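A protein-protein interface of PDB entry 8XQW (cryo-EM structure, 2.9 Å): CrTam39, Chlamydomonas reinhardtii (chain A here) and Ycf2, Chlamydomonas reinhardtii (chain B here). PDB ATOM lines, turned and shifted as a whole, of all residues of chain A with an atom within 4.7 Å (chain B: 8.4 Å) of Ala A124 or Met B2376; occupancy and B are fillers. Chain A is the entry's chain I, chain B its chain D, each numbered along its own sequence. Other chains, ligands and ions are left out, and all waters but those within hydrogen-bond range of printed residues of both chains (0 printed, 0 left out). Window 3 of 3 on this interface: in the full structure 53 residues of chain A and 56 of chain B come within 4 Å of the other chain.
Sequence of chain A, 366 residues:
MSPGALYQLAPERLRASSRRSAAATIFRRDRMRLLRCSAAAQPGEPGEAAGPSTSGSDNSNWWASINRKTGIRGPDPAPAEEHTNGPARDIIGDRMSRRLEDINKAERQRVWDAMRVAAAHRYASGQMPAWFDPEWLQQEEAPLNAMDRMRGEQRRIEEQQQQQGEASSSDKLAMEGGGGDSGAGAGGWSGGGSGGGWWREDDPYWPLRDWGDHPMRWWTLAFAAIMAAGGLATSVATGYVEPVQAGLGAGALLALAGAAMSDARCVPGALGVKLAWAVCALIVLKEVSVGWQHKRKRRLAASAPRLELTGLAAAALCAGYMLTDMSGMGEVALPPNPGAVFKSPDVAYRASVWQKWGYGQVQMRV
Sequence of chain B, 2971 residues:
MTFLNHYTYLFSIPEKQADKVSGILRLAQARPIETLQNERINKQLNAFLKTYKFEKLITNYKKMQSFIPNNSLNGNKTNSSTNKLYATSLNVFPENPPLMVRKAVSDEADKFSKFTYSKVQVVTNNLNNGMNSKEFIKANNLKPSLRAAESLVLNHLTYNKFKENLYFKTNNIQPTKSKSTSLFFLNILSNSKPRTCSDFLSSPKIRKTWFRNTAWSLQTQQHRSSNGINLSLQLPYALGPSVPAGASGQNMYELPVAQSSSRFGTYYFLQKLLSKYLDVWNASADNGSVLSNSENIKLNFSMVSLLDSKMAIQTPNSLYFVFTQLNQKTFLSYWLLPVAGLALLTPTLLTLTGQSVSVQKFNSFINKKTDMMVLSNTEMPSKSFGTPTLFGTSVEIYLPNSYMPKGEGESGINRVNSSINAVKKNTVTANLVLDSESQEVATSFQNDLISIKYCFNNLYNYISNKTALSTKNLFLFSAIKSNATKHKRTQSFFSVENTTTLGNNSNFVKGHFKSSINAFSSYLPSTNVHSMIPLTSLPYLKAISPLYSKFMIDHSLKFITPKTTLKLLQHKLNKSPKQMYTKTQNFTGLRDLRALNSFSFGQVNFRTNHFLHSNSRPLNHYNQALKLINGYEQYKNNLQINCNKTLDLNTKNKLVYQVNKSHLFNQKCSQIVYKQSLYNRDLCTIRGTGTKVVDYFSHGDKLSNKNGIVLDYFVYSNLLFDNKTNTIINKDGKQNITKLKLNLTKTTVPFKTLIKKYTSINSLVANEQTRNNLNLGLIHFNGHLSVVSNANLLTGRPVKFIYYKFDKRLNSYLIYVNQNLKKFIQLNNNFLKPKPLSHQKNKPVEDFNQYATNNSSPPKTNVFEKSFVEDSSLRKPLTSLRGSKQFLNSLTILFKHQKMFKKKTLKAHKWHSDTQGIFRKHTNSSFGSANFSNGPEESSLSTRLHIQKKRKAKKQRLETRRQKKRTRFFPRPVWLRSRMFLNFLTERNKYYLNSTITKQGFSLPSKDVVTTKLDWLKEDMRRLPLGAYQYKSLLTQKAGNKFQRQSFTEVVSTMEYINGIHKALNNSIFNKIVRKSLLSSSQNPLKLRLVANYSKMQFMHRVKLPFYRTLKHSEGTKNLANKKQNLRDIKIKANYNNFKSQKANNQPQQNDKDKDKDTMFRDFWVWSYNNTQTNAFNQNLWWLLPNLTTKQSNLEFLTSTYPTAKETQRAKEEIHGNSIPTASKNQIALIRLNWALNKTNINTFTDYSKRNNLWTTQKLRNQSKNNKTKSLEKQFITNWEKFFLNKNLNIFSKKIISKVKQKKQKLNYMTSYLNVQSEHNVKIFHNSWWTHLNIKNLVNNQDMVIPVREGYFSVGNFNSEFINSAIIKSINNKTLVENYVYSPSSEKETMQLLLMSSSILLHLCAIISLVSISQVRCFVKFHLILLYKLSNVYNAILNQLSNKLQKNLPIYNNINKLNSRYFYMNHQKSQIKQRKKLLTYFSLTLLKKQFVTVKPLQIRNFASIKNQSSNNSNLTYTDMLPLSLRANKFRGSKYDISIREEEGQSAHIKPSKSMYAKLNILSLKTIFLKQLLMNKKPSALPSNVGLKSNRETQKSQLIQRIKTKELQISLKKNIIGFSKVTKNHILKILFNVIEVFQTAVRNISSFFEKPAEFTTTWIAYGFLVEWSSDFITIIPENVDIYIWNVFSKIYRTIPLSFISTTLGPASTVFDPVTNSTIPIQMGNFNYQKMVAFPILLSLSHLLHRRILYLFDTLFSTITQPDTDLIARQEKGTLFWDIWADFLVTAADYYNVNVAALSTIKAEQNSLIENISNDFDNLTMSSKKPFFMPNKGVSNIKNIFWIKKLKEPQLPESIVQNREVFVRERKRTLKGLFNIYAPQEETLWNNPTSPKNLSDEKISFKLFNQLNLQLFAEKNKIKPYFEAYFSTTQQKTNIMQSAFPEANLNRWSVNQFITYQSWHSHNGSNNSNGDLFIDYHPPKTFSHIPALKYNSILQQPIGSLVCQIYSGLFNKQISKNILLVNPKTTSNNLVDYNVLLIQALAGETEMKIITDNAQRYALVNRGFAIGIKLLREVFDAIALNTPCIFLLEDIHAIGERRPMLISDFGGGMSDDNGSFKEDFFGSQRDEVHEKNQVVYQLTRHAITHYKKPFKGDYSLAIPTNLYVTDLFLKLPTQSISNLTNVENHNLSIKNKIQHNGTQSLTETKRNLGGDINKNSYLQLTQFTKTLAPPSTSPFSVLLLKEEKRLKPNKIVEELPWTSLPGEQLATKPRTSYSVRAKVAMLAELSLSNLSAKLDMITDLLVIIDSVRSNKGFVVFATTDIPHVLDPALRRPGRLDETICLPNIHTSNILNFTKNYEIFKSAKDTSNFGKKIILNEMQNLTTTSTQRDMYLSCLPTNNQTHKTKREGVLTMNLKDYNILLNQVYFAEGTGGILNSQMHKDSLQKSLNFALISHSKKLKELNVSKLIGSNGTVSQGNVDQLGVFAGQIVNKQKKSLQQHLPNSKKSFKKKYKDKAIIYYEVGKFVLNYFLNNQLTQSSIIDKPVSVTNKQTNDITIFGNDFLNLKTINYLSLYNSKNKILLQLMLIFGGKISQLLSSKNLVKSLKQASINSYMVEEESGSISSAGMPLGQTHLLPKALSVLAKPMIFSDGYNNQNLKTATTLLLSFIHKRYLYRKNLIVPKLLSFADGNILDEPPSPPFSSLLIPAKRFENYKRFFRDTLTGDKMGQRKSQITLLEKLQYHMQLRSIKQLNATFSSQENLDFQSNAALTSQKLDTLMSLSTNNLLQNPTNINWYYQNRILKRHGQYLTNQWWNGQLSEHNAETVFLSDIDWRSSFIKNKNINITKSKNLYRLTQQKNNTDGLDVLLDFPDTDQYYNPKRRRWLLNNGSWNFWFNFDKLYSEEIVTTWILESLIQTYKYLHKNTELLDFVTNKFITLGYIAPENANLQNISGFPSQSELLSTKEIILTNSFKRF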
ATOM      1  N   ALA A 120     -30.658   1.498 -18.156  1.00  0.00           N
ATOM      2  CA  ALA A 120     -29.585   0.745 -18.789  1.00  0.00           C
ATOM      3  C   ALA A 120     -30.109  -0.046 -19.967  1.00  0.00           C
ATOM      4  O   ALA A 120     -29.503  -0.055 -21.041  1.00  0.00           O
ATOM      5  CB  ALA A 120     -28.932  -0.191 -17.782  1.00  0.00           C
ATOM      6  N   HIS A 121     -31.247  -0.706 -19.789  1.00  0.00           N
ATOM      7  CA  HIS A 121     -31.805  -1.477 -20.892  1.00  0.00           C
ATOM      8  C   HIS A 121     -32.206  -0.586 -22.053  1.00  0.00           C
ATOM      9  O   HIS A 121     -31.796  -0.820 -23.191  1.00  0.00           O
ATOM     10  CB  HIS A 121     -32.987  -2.292 -20.418  1.00  0.00           C
ATOM     11  CG  HIS A 121     -32.621  -3.678 -20.017  1.00  0.00           C
ATOM     12  ND1 HIS A 121     -32.570  -4.080 -18.703  1.00  0.00           N
ATOM     13  CD2 HIS A 121     -32.259  -4.750 -20.755  1.00  0.00           C
ATOM     14  CE1 HIS A 121     -32.208  -5.348 -18.648  1.00  0.00           C
ATOM     15  NE2 HIS A 121     -32.016  -5.778 -19.880  1.00  0.00           N
ATOM     16  N   ARG A 122     -33.004   0.448 -21.795  1.00  0.00           N
ATOM     17  CA  ARG A 122     -33.444   1.320 -22.878  1.00  0.00           C
ATOM     18  C   ARG A 122     -32.275   1.982 -23.579  1.00  0.00           C
ATOM     19  O   ARG A 122     -32.383   2.367 -24.743  1.00  0.00           O
ATOM     20  CB  ARG A 122     -34.383   2.385 -22.340  1.00  0.00           C
ATOM     21  CG  ARG A 122     -35.807   1.988 -22.387  1.00  0.00           C
ATOM     22  CD  ARG A 122     -36.633   2.919 -21.581  1.00  0.00           C
ATOM     23  NE  ARG A 122     -37.477   2.159 -20.683  1.00  0.00           N
ATOM     24  CZ  ARG A 122     -38.757   2.400 -20.485  1.00  0.00           C
ATOM     25  NH1 ARG A 122     -39.342   3.395 -21.118  1.00  0.00           N
ATOM     26  NH2 ARG A 122     -39.445   1.650 -19.647  1.00  0.00           N
ATOM     27  N   TYR A 123     -31.154   2.149 -22.890  1.00  0.00           N
ATOM     28  CA  TYR A 123     -30.025   2.819 -23.510  1.00  0.00           C
ATOM     29  C   TYR A 123     -29.231   1.856 -24.368  1.00  0.00           C
ATOM     30  O   TYR A 123     -28.786   2.215 -25.461  1.00  0.00           O
ATOM     31  CB  TYR A 123     -29.148   3.430 -22.435  1.00  0.00           C
ATOM     32  CG  TYR A 123     -27.809   3.890 -22.916  1.00  0.00           C
ATOM     33  CD1 TYR A 123     -27.683   5.022 -23.689  1.00  0.00           C
ATOM     34  CD2 TYR A 123     -26.665   3.206 -22.573  1.00  0.00           C
ATOM     35  CE1 TYR A 123     -26.461   5.448 -24.115  1.00  0.00           C
ATOM     36  CE2 TYR A 123     -25.442   3.625 -22.995  1.00  0.00           C
ATOM     37  CZ  TYR A 123     -25.345   4.745 -23.767  1.00  0.00           C
ATOM     38  OH  TYR A 123     -24.115   5.171 -24.192  1.00  0.00           O
ATOM     39  N   ALA A 124     -29.054   0.625 -23.897  1.00  0.00           N
ATOM     40  CA  ALA A 124     -28.317  -0.367 -24.662  1.00  0.00           C
ATOM     41  C   ALA A 124     -28.959  -0.670 -26.001  1.00  0.00           C
ATOM     42  O   ALA A 124     -28.298  -1.250 -26.863  1.00  0.00           O
ATOM     43  CB  ALA A 124     -28.182  -1.652 -23.859  1.00  0.00           C
ATOM     44  N   SER A 125     -30.215  -0.287 -26.205  1.00  0.00           N
ATOM     45  CA  SER A 125     -30.914  -0.563 -27.450  1.00  0.00           C
ATOM     46  C   SER A 125     -31.374   0.707 -28.149  1.00  0.00           C
ATOM     47  O   SER A 125     -32.395   0.692 -28.832  1.00  0.00           O
ATOM     48  CB  SER A 125     -32.104  -1.479 -27.200  1.00  0.00           C
ATOM     49  OG  SER A 125     -33.295  -0.727 -27.169  1.00  0.00           O
ATOM     50  N   GLY A 126     -30.667   1.814 -27.965  1.00  0.00           N
ATOM     51  CA  GLY A 126     -30.903   2.996 -28.766  1.00  0.00           C
ATOM     52  C   GLY A 126     -31.871   4.027 -28.221  1.00  0.00           C
ATOM     53  O   GLY A 126     -31.597   5.224 -28.300  1.00  0.00           O
ATOM     54  N   LEU A 137     -25.707   6.346 -14.225  1.00  0.00           N
ATOM     55  CA  LEU A 137     -25.967   4.981 -13.800  1.00  0.00           C
ATOM     56  C   LEU A 137     -24.971   4.492 -12.775  1.00  0.00           C
ATOM     57  O   LEU A 137     -25.114   3.371 -12.287  1.00  0.00           O
ATOM     58  CB  LEU A 137     -25.959   4.047 -15.002  1.00  0.00           C
ATOM     59  CG  LEU A 137     -26.927   4.390 -16.121  1.00  0.00           C
ATOM     60  CD1 LEU A 137     -26.672   3.510 -17.307  1.00  0.00           C
ATOM     61  CD2 LEU A 137     -28.338   4.222 -15.659  1.00  0.00           C
ATOM     62  N   SER B 275     -15.417   5.104 -24.245  1.00  0.00           N
ATOM     63  CA  SER B 275     -16.787   4.703 -24.520  1.00  0.00           C
ATOM     64  C   SER B 275     -17.626   5.884 -24.971  1.00  0.00           C
ATOM     65  O   SER B 275     -18.562   5.717 -25.756  1.00  0.00           O
ATOM     66  CB  SER B 275     -17.408   4.060 -23.291  1.00  0.00           C
ATOM     67  OG  SER B 275     -18.812   4.214 -23.330  1.00  0.00           O
ATOM     68  N   LYS B 276     -17.320   7.085 -24.483  1.00  0.00           N
ATOM     69  CA  LYS B 276     -18.050   8.244 -24.979  1.00  0.00           C
ATOM     70  C   LYS B 276     -17.739   8.520 -26.441  1.00  0.00           C
ATOM     71  O   LYS B 276     -18.653   8.773 -27.229  1.00  0.00           O
ATOM     72  CB  LYS B 276     -17.729   9.474 -24.139  1.00  0.00           C
ATOM     73  CG  LYS B 276     -18.031  10.780 -24.820  1.00  0.00           C
ATOM     74  CD  LYS B 276     -17.461  11.926 -24.021  1.00  0.00           C
ATOM     75  CE  LYS B 276     -17.550  13.221 -24.796  1.00  0.00           C
ATOM     76  NZ  LYS B 276     -17.042  14.378 -24.016  1.00  0.00           N
ATOM     77  N   ASP B 279     -18.790   5.035 -29.355  1.00  0.00           N
ATOM     78  CA  ASP B 279     -20.105   4.469 -29.622  1.00  0.00           C
ATOM     79  C   ASP B 279     -21.170   5.549 -29.757  1.00  0.00           C
ATOM     80  O   ASP B 279     -22.301   5.394 -29.289  1.00  0.00           O
ATOM     81  CB  ASP B 279     -20.491   3.466 -28.541  1.00  0.00           C
ATOM     82  CG  ASP B 279     -20.027   2.061 -28.863  1.00  0.00           C
ATOM     83  OD1 ASP B 279     -20.078   1.680 -30.052  1.00  0.00           O
ATOM     84  OD2 ASP B 279     -19.619   1.336 -27.933  1.00  0.00           O
ATOM     85  N   LYS B2370     -29.403  -6.422 -11.854  1.00  0.00           N
ATOM     86  CA  LYS B2370     -28.440  -5.343 -11.924  1.00  0.00           C
ATOM     87  C   LYS B2370     -27.216  -5.685 -12.745  1.00  0.00           C
ATOM     88  O   LYS B2370     -26.333  -4.838 -12.889  1.00  0.00           O
ATOM     89  CB  LYS B2370     -27.988  -4.954 -10.529  1.00  0.00           C
ATOM     90  CG  LYS B2370     -29.069  -4.431  -9.657  1.00  0.00           C
ATOM     91  CD  LYS B2370     -28.471  -3.787  -8.447  1.00  0.00           C
ATOM     92  CE  LYS B2370     -29.448  -2.851  -7.818  1.00  0.00           C
ATOM     93  NZ  LYS B2370     -30.719  -3.555  -7.551  1.00  0.00           N
ATOM     94  N   ILE B2371     -27.121  -6.900 -13.278  1.00  0.00           N
ATOM     95  CA  ILE B2371     -25.923  -7.259 -14.020  1.00  0.00           C
ATOM     96  C   ILE B2371     -25.831  -6.463 -15.307  1.00  0.00           C
ATOM     97  O   ILE B2371     -24.736  -6.238 -15.829  1.00  0.00           O
ATOM     98  CB  ILE B2371     -25.889  -8.772 -14.275  1.00  0.00           C
ATOM     99  CG1 ILE B2371     -24.605  -9.157 -14.991  1.00  0.00           C
ATOM    100  CG2 ILE B2371     -27.088  -9.194 -15.070  1.00  0.00           C
ATOM    101  CD1 ILE B2371     -23.979 -10.384 -14.451  1.00  0.00           C
ATOM    102  N   ILE B2372     -26.959  -5.977 -15.817  1.00  0.00           N
ATOM    103  CA  ILE B2372     -26.929  -5.140 -17.008  1.00  0.00           C
ATOM    104  C   ILE B2372     -26.139  -3.877 -16.749  1.00  0.00           C
ATOM    105  O   ILE B2372     -25.653  -3.237 -17.683  1.00  0.00           O
ATOM    106  CB  ILE B2372     -28.361  -4.828 -17.469  1.00  0.00           C
ATOM    107  CG1 ILE B2372     -28.356  -3.993 -18.740  1.00  0.00           C
ATOM    108  CG2 ILE B2372     -29.096  -4.096 -16.403  1.00  0.00           C
ATOM    109  CD1 ILE B2372     -27.701  -4.644 -19.896  1.00  0.00           C
ATOM    110  N   LEU B2373     -25.973  -3.502 -15.492  1.00  0.00           N
ATOM    111  CA  LEU B2373     -25.237  -2.283 -15.218  1.00  0.00           C
ATOM    112  C   LEU B2373     -23.740  -2.482 -15.291  1.00  0.00           C
ATOM    113  O   LEU B2373     -22.999  -1.520 -15.091  1.00  0.00           O
ATOM    114  CB  LEU B2373     -25.624  -1.731 -13.852  1.00  0.00           C
ATOM    115  CG  LEU B2373     -26.998  -1.072 -13.797  1.00  0.00           C
ATOM    116  CD1 LEU B2373     -27.485  -1.065 -12.395  1.00  0.00           C
ATOM    117  CD2 LEU B2373     -26.930   0.322 -14.317  1.00  0.00           C
ATOM    118  N   ASN B2374     -23.280  -3.701 -15.566  1.00  0.00           N
ATOM    119  CA  ASN B2374     -21.868  -4.000 -15.760  1.00  0.00           C
ATOM    120  C   ASN B2374     -21.560  -4.373 -17.198  1.00  0.00           C
ATOM    121  O   ASN B2374     -20.533  -4.990 -17.463  1.00  0.00           O
ATOM    122  CB  ASN B2374     -21.422  -5.132 -14.844  1.00  0.00           C
ATOM    123  CG  ASN B2374     -21.421  -4.744 -13.403  1.00  0.00           C
ATOM    124  OD1 ASN B2374     -20.685  -3.863 -12.984  1.00  0.00           O
ATOM    125  ND2 ASN B2374     -22.238  -5.413 -12.623  1.00  0.00           N
ATOM    126  N   GLU B2375     -22.438  -4.026 -18.132  1.00  0.00           N
ATOM    127  CA  GLU B2375     -22.256  -4.379 -19.529  1.00  0.00           C
ATOM    128  C   GLU B2375     -22.446  -3.196 -20.458  1.00  0.00           C
ATOM    129  O   GLU B2375     -22.677  -3.397 -21.649  1.00  0.00           O
ATOM    130  CB  GLU B2375     -23.225  -5.485 -19.927  1.00  0.00           C
ATOM    131  CG  GLU B2375     -23.540  -6.430 -18.822  1.00  0.00           C
ATOM    132  CD  GLU B2375     -24.215  -7.674 -19.308  1.00  0.00           C
ATOM    133  OE1 GLU B2375     -24.581  -7.720 -20.493  1.00  0.00           O
ATOM    134  OE2 GLU B2375     -24.377  -8.614 -18.510  1.00  0.00           O
ATOM    135  N   MET B2376     -22.367  -1.973 -19.954  1.00  0.00           N
ATOM    136  CA  MET B2376     -22.645  -0.808 -20.775  1.00  0.00           C
ATOM    137  C   MET B2376     -21.486  -0.418 -21.668  1.00  0.00           C
ATOM    138  O   MET B2376     -21.683   0.363 -22.599  1.00  0.00           O
ATOM    139  CB  MET B2376     -23.023   0.369 -19.887  1.00  0.00           C
ATOM    140  CG  MET B2376     -24.257   0.134 -19.070  1.00  0.00           C
ATOM    141  SD  MET B2376     -25.746   0.423 -20.019  1.00  0.00           S
ATOM    142  CE  MET B2376     -26.121  -1.230 -20.572  1.00  0.00           C
ATOM    143  N   GLN B2377     -20.289  -0.921 -21.409  1.00  0.00           N
ATOM    144  CA  GLN B2377     -19.132  -0.659 -22.250  1.00  0.00           C
ATOM    145  C   GLN B2377     -18.603  -1.991 -22.742  1.00  0.00           C
ATOM    146  O   GLN B2377     -18.008  -2.750 -21.974  1.00  0.00           O
ATOM    147  CB  GLN B2377     -18.039   0.087 -21.498  1.00  0.00           C
ATOM    148  CG  GLN B2377     -18.512   1.221 -20.663  1.00  0.00           C
ATOM    149  CD  GLN B2377     -17.381   1.844 -19.918  1.00  0.00           C
ATOM    150  OE1 GLN B2377     -16.229   1.548 -20.178  1.00  0.00           O
ATOM    151  NE2 GLN B2377     -17.697   2.709 -18.977  1.00  0.00           N
ATOM    152  N   ASN B2378     -18.818  -2.276 -24.017  1.00  0.00           N
ATOM    153  CA  ASN B2378     -18.222  -3.447 -24.637  1.00  0.00           C
ATOM    154  C   ASN B2378     -18.048  -3.132 -26.106  1.00  0.00           C
ATOM    155  O   ASN B2378     -19.023  -2.826 -26.794  1.00  0.00           O
ATOM    156  CB  ASN B2378     -19.081  -4.694 -24.437  1.00  0.00           C
ATOM    157  CG  ASN B2378     -20.537  -4.441 -24.712  1.00  0.00           C
ATOM    158  OD1 ASN B2378     -20.947  -3.302 -24.917  1.00  0.00           O
ATOM    159  ND2 ASN B2378     -21.336  -5.500 -24.700  1.00  0.00           N
ATOM    160  N   LEU B2379     -16.809  -3.183 -26.573  1.00  0.00           N
ATOM    161  CA  LEU B2379     -16.502  -2.795 -27.939  1.00  0.00           C
ATOM    162  C   LEU B2379     -16.711  -3.919 -28.939  1.00  0.00           C
ATOM    163  O   LEU B2379     -16.109  -3.890 -30.017  1.00  0.00           O
ATOM    164  CB  LEU B2379     -15.073  -2.264 -28.021  1.00  0.00           C
ATOM    165  CG  LEU B2379     -14.891  -0.827 -27.529  1.00  0.00           C
ATOM    166  CD1 LEU B2379     -15.922   0.060 -28.181  1.00  0.00           C
ATOM    167  CD2 LEU B2379     -14.984  -0.716 -26.025  1.00  0.00           C
ATOM    168  N   LYS B2403     -33.784  -5.274 -24.456  1.00  0.00           N
ATOM    169  CA  LYS B2403     -34.720  -6.380 -24.629  1.00  0.00           C
ATOM    170  C   LYS B2403     -35.966  -6.234 -23.752  1.00  0.00           C
ATOM    171  O   LYS B2403     -36.880  -5.480 -24.077  1.00  0.00           O
ATOM    172  CB  LYS B2403     -34.030  -7.712 -24.325  1.00  0.00           C
ATOM    173  CG  LYS B2403     -32.953  -8.106 -25.318  1.00  0.00           C
ATOM    174  CD  LYS B2403     -33.540  -8.367 -26.686  1.00  0.00           C
ATOM    175  CE  LYS B2403     -32.455  -8.651 -27.701  1.00  0.00           C
ATOM    176  NZ  LYS B2403     -33.011  -8.739 -29.078  1.00  0.00           N
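Ala A120 touches Ile B2372 (CB to CG1, 3.96 Å).
CE of Met B2376 touches O of Ala A120, at 3.6 Å.
SD of Met B2376 touches CD2 of Tyr A123, at 3.9 Å.
Met B2376 touches Ala A124 (CE to CB, 3.9 Å).
Leu A137 touches Leu B2373.
Hydrophobic or aromatic side chains of chain A that line the printed part of chain B: Ala A120, Tyr A123, Ala A124 and Leu A137.
Hydrophobic or aromatic side chains of chain B that line the printed part of chain A: Ile B2372, Leu B2373 and Met B2376.
Among the printed residues, no Asp or Glu carboxylate lies within 4 Å of a Lys or Arg side-chain nitrogen of the other chain.
Printed residues of chain B within 4 Å of Tyr A123: Met B2376.
Of chain B, only Met B2376 comes within 4 Å of Ala A124.
Of the printed residues of chain A, Ile B2372 touches Ala A120.
Of the printed residues of chain A, Leu B2373 touches Leu A137 (3.9 Å).
Of chain A, only Ala A120 (3.6 Å), Tyr A123 (3.9 Å) and Ala A124 (3.9 Å) come within 4 Å of Met B2376.
The nearest residue of chain A that does not touch Met B2376 is Leu A137 (4.2 Å).
The nearest printed residue of chain B that does not touch Ala A120 is Leu B2373 (4.03 Å).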
